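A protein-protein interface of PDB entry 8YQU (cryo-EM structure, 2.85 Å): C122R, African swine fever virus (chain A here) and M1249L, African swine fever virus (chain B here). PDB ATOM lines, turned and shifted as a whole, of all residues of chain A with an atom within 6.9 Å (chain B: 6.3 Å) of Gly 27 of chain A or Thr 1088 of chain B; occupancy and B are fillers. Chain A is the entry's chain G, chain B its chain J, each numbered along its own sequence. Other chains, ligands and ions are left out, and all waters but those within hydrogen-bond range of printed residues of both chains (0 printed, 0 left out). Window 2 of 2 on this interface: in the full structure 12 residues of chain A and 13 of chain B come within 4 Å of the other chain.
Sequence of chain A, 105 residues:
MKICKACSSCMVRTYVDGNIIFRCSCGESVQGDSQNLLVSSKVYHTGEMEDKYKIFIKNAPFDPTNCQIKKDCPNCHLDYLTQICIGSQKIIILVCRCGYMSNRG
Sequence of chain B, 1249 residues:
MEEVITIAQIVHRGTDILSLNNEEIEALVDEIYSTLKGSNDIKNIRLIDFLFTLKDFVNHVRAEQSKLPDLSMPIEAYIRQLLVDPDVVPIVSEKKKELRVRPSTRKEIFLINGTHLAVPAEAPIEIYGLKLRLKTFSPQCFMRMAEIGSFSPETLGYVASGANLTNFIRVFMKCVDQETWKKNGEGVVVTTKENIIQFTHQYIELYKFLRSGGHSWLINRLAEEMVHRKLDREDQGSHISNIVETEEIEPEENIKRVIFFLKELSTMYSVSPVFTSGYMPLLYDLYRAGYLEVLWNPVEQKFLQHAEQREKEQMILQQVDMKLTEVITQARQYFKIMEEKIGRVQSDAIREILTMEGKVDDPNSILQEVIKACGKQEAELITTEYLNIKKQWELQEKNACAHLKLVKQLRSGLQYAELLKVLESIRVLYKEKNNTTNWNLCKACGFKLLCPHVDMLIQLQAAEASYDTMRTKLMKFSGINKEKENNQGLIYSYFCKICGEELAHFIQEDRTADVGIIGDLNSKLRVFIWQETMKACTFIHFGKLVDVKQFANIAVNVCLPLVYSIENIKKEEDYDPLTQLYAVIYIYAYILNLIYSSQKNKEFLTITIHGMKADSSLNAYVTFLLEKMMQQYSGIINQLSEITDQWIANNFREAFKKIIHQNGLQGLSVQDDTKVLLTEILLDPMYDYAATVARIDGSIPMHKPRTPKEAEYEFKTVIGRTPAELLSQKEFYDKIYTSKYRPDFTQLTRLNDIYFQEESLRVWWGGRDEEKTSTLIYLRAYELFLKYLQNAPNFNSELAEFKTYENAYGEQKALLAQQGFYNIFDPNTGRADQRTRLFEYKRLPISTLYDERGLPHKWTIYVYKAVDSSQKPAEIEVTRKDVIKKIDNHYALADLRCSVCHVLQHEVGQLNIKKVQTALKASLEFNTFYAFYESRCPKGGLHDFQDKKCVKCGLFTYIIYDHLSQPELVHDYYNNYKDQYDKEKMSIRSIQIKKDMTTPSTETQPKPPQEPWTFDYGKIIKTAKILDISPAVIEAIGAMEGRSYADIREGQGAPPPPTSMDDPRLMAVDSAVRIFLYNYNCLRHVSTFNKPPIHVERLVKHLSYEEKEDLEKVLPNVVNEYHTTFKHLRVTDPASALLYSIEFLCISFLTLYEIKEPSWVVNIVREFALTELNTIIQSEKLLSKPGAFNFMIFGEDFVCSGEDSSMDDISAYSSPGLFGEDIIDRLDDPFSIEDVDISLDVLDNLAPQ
Of chain B, only His 1085 (3.4 Å) and Thr 1088 (3.9 Å) come within 4 Å of Gly 27 of chain A. Printed residues of chain A within 4 Å of Thr 1088 of chain B: Gly 27. Of the printed residues of chain B, Ser 25 of chain A touches Phe 1089 (3.5 Å). Printed residues of chain A within 4 Å of Asn 1081 of chain B: Cys 26. Of the printed residues of chain A, Cys 1082 of chain B touches Cys 26. Printed residues of chain A within 4 Å of His 1085 of chain B: Gly 27 and Glu 28. Asn 1090 of chain B touches none of the printed residues of chain A. Cys 24 of chain A touches none of the printed residues of chain B. The nearest residue of chain A that does not touch Thr 1088 of chain B is Arg 23 of chain A (5.5 Å). The nearest printed residue of chain B that does not touch Glu 28 of chain A is Asn 1081 of chain B (4.3 Å).
The side-chain hydroxyl (OG1) of Thr 1088 of chain B is in hydrogen-bond range of the backbone carbonyl oxygen (O) of His 1085 of chain B. A ring nitrogen (ND1) of His 1085 of chain B sits at hydrogen-bond distance from the backbone carbonyl oxygen (O) of Asn 1081 of chain B.
Of the 10 printed residues of chain A, 4 touch a printed residue of chain B. Printed residues of chain A that touch a printed residue of chain B: Ser 25, Cys 26, Gly 27 and Glu 28. Of the 9 printed residues of chain B, 5 touch a printed residue of chain A. Hydrophobic or aromatic side chains of chain B that line the printed part of chain A: His 1085 and Phe 1089. Among the printed residues, 7 pairs touch across the chains. Among the printed residues, no Asp or Glu carboxylate lies within 4 Å of a Lys or Arg side-chain nitrogen of the other chain.
Phe 1089 of chain B touches Ser 25 of chain A. Cys 1082 of chain B touches Cys 26 of chain A. C of Cys 26 of chain A touches CZ of Phe 1089 of chain B (3.97 Å). O of Gly 27 of chain A touches CG of His 1085 of chain B, 3.4 Å away. OG1 of Thr 1088 of chain B touches CA of Gly 27 of chain A, at 3.9 Å. OE1 of Glu 28 of chain A touches CE1 of His 1085 of chain B, 3.5 Å away.
O of Asn 1081 of chain B lies close to O of Cys 26 of chain A (3.1 Å).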
ATOM      1  N   CYS A   4     -21.014  17.647  13.598  1.00  0.00           N
ATOM      2  CA  CYS A   4     -21.465  16.346  13.127  1.00  0.00           C
ATOM      3  C   CYS A   4     -20.893  16.044  11.747  1.00  0.00           C
ATOM      4  O   CYS A   4     -20.879  16.900  10.860  1.00  0.00           O
ATOM      5  CB  CYS A   4     -22.993  16.307  13.086  1.00  0.00           C
ATOM      6  SG  CYS A   4     -23.704  14.709  12.642  1.00  0.00           S
ATOM      7  N   MET A  11     -23.169  19.537  17.561  1.00  0.00           N
ATOM      8  CA  MET A  11     -23.624  18.428  18.385  1.00  0.00           C
ATOM      9  C   MET A  11     -23.702  18.839  19.851  1.00  0.00           C
ATOM     10  O   MET A  11     -22.944  19.692  20.321  1.00  0.00           O
ATOM     11  CB  MET A  11     -22.690  17.228  18.217  1.00  0.00           C
ATOM     12  CG  MET A  11     -22.719  16.636  16.818  1.00  0.00           C
ATOM     13  SD  MET A  11     -21.568  15.273  16.578  1.00  0.00           S
ATOM     14  CE  MET A  11     -22.357  13.997  17.550  1.00  0.00           C
ATOM     15  N   ARG A  23     -24.010  13.986  21.082  1.00  0.00           N
ATOM     16  CA  ARG A  23     -25.171  13.449  20.392  1.00  0.00           C
ATOM     17  C   ARG A  23     -25.797  14.555  19.559  1.00  0.00           C
ATOM     18  O   ARG A  23     -25.954  15.685  20.030  1.00  0.00           O
ATOM     19  CB  ARG A  23     -26.193  12.878  21.383  1.00  0.00           C
ATOM     20  CG  ARG A  23     -27.205  11.934  20.757  1.00  0.00           C
ATOM     21  CD  ARG A  23     -28.131  11.342  21.806  1.00  0.00           C
ATOM     22  NE  ARG A  23     -27.410  10.524  22.774  1.00  0.00           N
ATOM     23  CZ  ARG A  23     -27.284  10.821  24.060  1.00  0.00           C
ATOM     24  NH1 ARG A  23     -27.824  11.914  24.574  1.00  0.00           N
ATOM     25  NH2 ARG A  23     -26.601   9.999  24.851  1.00  0.00           N
ATOM     26  N   CYS A  24     -26.146  14.227  18.322  1.00  0.00           N
ATOM     27  CA  CYS A  24     -26.680  15.197  17.381  1.00  0.00           C
ATOM     28  C   CYS A  24     -28.191  15.041  17.245  1.00  0.00           C
ATOM     29  O   CYS A  24     -28.792  14.077  17.723  1.00  0.00           O
ATOM     30  CB  CYS A  24     -26.002  15.043  16.016  1.00  0.00           C
ATOM     31  SG  CYS A  24     -26.412  16.337  14.831  1.00  0.00           S
ATOM     32  N   SER A  25     -28.804  16.017  16.574  1.00  0.00           N
ATOM     33  CA  SER A  25     -30.236  15.978  16.318  1.00  0.00           C
ATOM     34  C   SER A  25     -30.612  14.977  15.234  1.00  0.00           C
ATOM     35  O   SER A  25     -31.803  14.696  15.060  1.00  0.00           O
ATOM     36  CB  SER A  25     -30.738  17.369  15.926  1.00  0.00           C
ATOM     37  OG  SER A  25     -32.125  17.348  15.639  1.00  0.00           O
ATOM     38  N   CYS A  26     -29.635  14.436  14.510  1.00  0.00           N
ATOM     39  CA  CYS A  26     -29.874  13.427  13.489  1.00  0.00           C
ATOM     40  C   CYS A  26     -29.598  12.016  13.991  1.00  0.00           C
ATOM     41  O   CYS A  26     -29.625  11.070  13.198  1.00  0.00           O
ATOM     42  CB  CYS A  26     -29.025  13.720  12.252  1.00  0.00           C
ATOM     43  SG  CYS A  26     -27.253  13.452  12.480  1.00  0.00           S
ATOM     44  N   GLY A  27     -29.332  11.853  15.286  1.00  0.00           N
ATOM     45  CA  GLY A  27     -29.090  10.552  15.866  1.00  0.00           C
ATOM     46  C   GLY A  27     -27.645  10.106  15.880  1.00  0.00           C
ATOM     47  O   GLY A  27     -27.332   9.101  16.531  1.00  0.00           O
ATOM     48  N   GLU A  28     -26.754  10.812  15.187  1.00  0.00           N
ATOM     49  CA  GLU A  28     -25.343  10.450  15.183  1.00  0.00           C
ATOM     50  C   GLU A  28     -24.730  10.749  16.546  1.00  0.00           C
ATOM     51  O   GLU A  28     -24.887  11.854  17.076  1.00  0.00           O
ATOM     52  CB  GLU A  28     -24.606  11.212  14.084  1.00  0.00           C
ATOM     53  CG  GLU A  28     -23.099  11.018  14.097  1.00  0.00           C
ATOM     54  CD  GLU A  28     -22.680   9.673  13.540  1.00  0.00           C
ATOM     55  OE1 GLU A  28     -23.366   9.165  12.629  1.00  0.00           O
ATOM     56  OE2 GLU A  28     -21.664   9.122  14.013  1.00  0.00           O
ATOM     57  N   SER A  29     -24.033   9.768  17.113  1.00  0.00           N
ATOM     58  CA  SER A  29     -23.399   9.910  18.417  1.00  0.00           C
ATOM     59  C   SER A  29     -21.931   9.535  18.306  1.00  0.00           C
ATOM     60  O   SER A  29     -21.595   8.485  17.748  1.00  0.00           O
ATOM     61  CB  SER A  29     -24.091   9.038  19.470  1.00  0.00           C
ATOM     62  OG  SER A  29     -23.804   7.666  19.262  1.00  0.00           O
ATOM     63  N   VAL A  30     -21.063  10.395  18.835  1.00  0.00           N
ATOM     64  CA  VAL A  30     -19.624  10.168  18.840  1.00  0.00           C
ATOM     65  C   VAL A  30     -19.112  10.519  20.233  1.00  0.00           C
ATOM     66  O   VAL A  30     -19.791  11.181  21.014  1.00  0.00           O
ATOM     67  CB  VAL A  30     -18.904  10.994  17.750  1.00  0.00           C
ATOM     68  CG1 VAL A  30     -19.005  12.484  18.048  1.00  0.00           C
ATOM     69  CG2 VAL A  30     -17.455  10.548  17.561  1.00  0.00           C
ATOM     70  N   ASN B1081     -29.826   9.795   8.083  1.00  0.00           N
ATOM     71  CA  ASN B1081     -29.266   9.361   9.356  1.00  0.00           C
ATOM     72  C   ASN B1081     -30.325   9.300  10.448  1.00  0.00           C
ATOM     73  O   ASN B1081     -30.165   8.555  11.420  1.00  0.00           O
ATOM     74  CB  ASN B1081     -28.119  10.284   9.764  1.00  0.00           C
ATOM     75  CG  ASN B1081     -26.846   9.993   8.999  1.00  0.00           C
ATOM     76  OD1 ASN B1081     -26.455  10.750   8.113  1.00  0.00           O
ATOM     77  ND2 ASN B1081     -26.194   8.887   9.336  1.00  0.00           N
ATOM     78  N   CYS B1082     -31.404  10.076  10.315  1.00  0.00           N
ATOM     79  CA  CYS B1082     -32.514   9.952  11.254  1.00  0.00           C
ATOM     80  C   CYS B1082     -33.147   8.570  11.164  1.00  0.00           C
ATOM     81  O   CYS B1082     -33.459   7.953  12.190  1.00  0.00           O
ATOM     82  CB  CYS B1082     -33.553  11.041  10.989  1.00  0.00           C
ATOM     83  SG  CYS B1082     -33.086  12.680  11.589  1.00  0.00           S
ATOM     84  N   HIS B1085     -30.545   6.038  12.605  1.00  0.00           N
ATOM     85  CA  HIS B1085     -30.453   5.997  14.060  1.00  0.00           C
ATOM     86  C   HIS B1085     -31.827   6.180  14.690  1.00  0.00           C
ATOM     87  O   HIS B1085     -31.975   6.920  15.667  1.00  0.00           O
ATOM     88  CB  HIS B1085     -29.493   7.075  14.568  1.00  0.00           C
ATOM     89  CG  HIS B1085     -28.089   6.916  14.075  1.00  0.00           C
ATOM     90  ND1 HIS B1085     -27.601   7.600  12.984  1.00  0.00           N
ATOM     91  CD2 HIS B1085     -27.066   6.151  14.528  1.00  0.00           C
ATOM     92  CE1 HIS B1085     -26.339   7.264  12.783  1.00  0.00           C
ATOM     93  NE2 HIS B1085     -25.991   6.386  13.707  1.00  0.00           N
ATOM     94  N   VAL B1086     -32.836   5.506  14.132  1.00  0.00           N
ATOM     95  CA  VAL B1086     -34.210   5.692  14.593  1.00  0.00           C
ATOM     96  C   VAL B1086     -34.372   5.213  16.032  1.00  0.00           C
ATOM     97  O   VAL B1086     -35.207   5.729  16.783  1.00  0.00           O
ATOM     98  CB  VAL B1086     -35.189   4.983  13.636  1.00  0.00           C
ATOM     99  CG1 VAL B1086     -34.970   3.476  13.655  1.00  0.00           C
ATOM    100  CG2 VAL B1086     -36.627   5.326  13.985  1.00  0.00           C
ATOM    101  N   SER B1087     -33.574   4.223  16.440  1.00  0.00           N
ATOM    102  CA  SER B1087     -33.710   3.669  17.784  1.00  0.00           C
ATOM    103  C   SER B1087     -33.335   4.679  18.862  1.00  0.00           C
ATOM    104  O   SER B1087     -33.962   4.705  19.926  1.00  0.00           O
ATOM    105  CB  SER B1087     -32.854   2.411  17.921  1.00  0.00           C
ATOM    106  OG  SER B1087     -31.487   2.697  17.688  1.00  0.00           O
ATOM    107  N   THR B1088     -32.321   5.511  18.611  1.00  0.00           N
ATOM    108  CA  THR B1088     -31.865   6.461  19.619  1.00  0.00           C
ATOM    109  C   THR B1088     -32.899   7.538  19.922  1.00  0.00           C
ATOM    110  O   THR B1088     -32.858   8.128  21.007  1.00  0.00           O
ATOM    111  CB  THR B1088     -30.558   7.117  19.171  1.00  0.00           C
ATOM    112  OG1 THR B1088     -30.740   7.717  17.883  1.00  0.00           O
ATOM    113  CG2 THR B1088     -29.444   6.082  19.090  1.00  0.00           C
ATOM    114  N   PHE B1089     -33.815   7.808  18.997  1.00  0.00           N
ATOM    115  CA  PHE B1089     -34.817   8.843  19.206  1.00  0.00           C
ATOM    116  C   PHE B1089     -35.814   8.437  20.286  1.00  0.00           C
ATOM    117  O   PHE B1089     -36.168   7.264  20.430  1.00  0.00           O
ATOM    118  CB  PHE B1089     -35.568   9.132  17.906  1.00  0.00           C
ATOM    119  CG  PHE B1089     -34.796   9.968  16.929  1.00  0.00           C
ATOM    120  CD1 PHE B1089     -33.902   9.382  16.050  1.00  0.00           C
ATOM    121  CD2 PHE B1089     -34.972  11.340  16.884  1.00  0.00           C
ATOM    122  CE1 PHE B1089     -33.192  10.149  15.149  1.00  0.00           C
ATOM    123  CE2 PHE B1089     -34.266  12.113  15.984  1.00  0.00           C
ATOM    124  CZ  PHE B1089     -33.375  11.517  15.116  1.00  0.00           C
ATOM    125  N   ASN B1090     -36.266   9.432  21.053  1.00  0.00           N
ATOM    126  CA  ASN B1090     -37.394   9.212  21.952  1.00  0.00           C
ATOM    127  C   ASN B1090     -38.645   8.856  21.162  1.00  0.00           C
ATOM    128  O   ASN B1090     -39.412   7.970  21.558  1.00  0.00           O
ATOM    129  CB  ASN B1090     -37.632  10.453  22.811  1.00  0.00           C
ATOM    130  CG  ASN B1090     -38.586  10.193  23.960  1.00  0.00           C
ATOM    131  OD1 ASN B1090     -38.936   9.049  24.246  1.00  0.00           O
ATOM    132  ND2 ASN B1090     -39.014  11.260  24.624  1.00  0.00           N
ATOM    133  N   LYS B1091     -38.866   9.542  20.039  1.00  0.00           N
ATOM    134  CA  LYS B1091     -39.886   9.200  19.068  1.00  0.00           C
ATOM    135  C   LYS B1091     -39.372   9.666  17.715  1.00  0.00           C
ATOM    136  O   LYS B1091     -38.803  10.765  17.621  1.00  0.00           O
ATOM    137  CB  LYS B1091     -41.246   9.839  19.377  1.00  0.00           C
ATOM    138  CG  LYS B1091     -41.253  11.358  19.400  1.00  0.00           C
ATOM    139  CD  LYS B1091     -42.664  11.896  19.559  1.00  0.00           C
ATOM    140  CE  LYS B1091     -43.508  11.599  18.329  1.00  0.00           C
ATOM    141  NZ  LYS B1091     -43.007  12.311  17.121  1.00  0.00           N
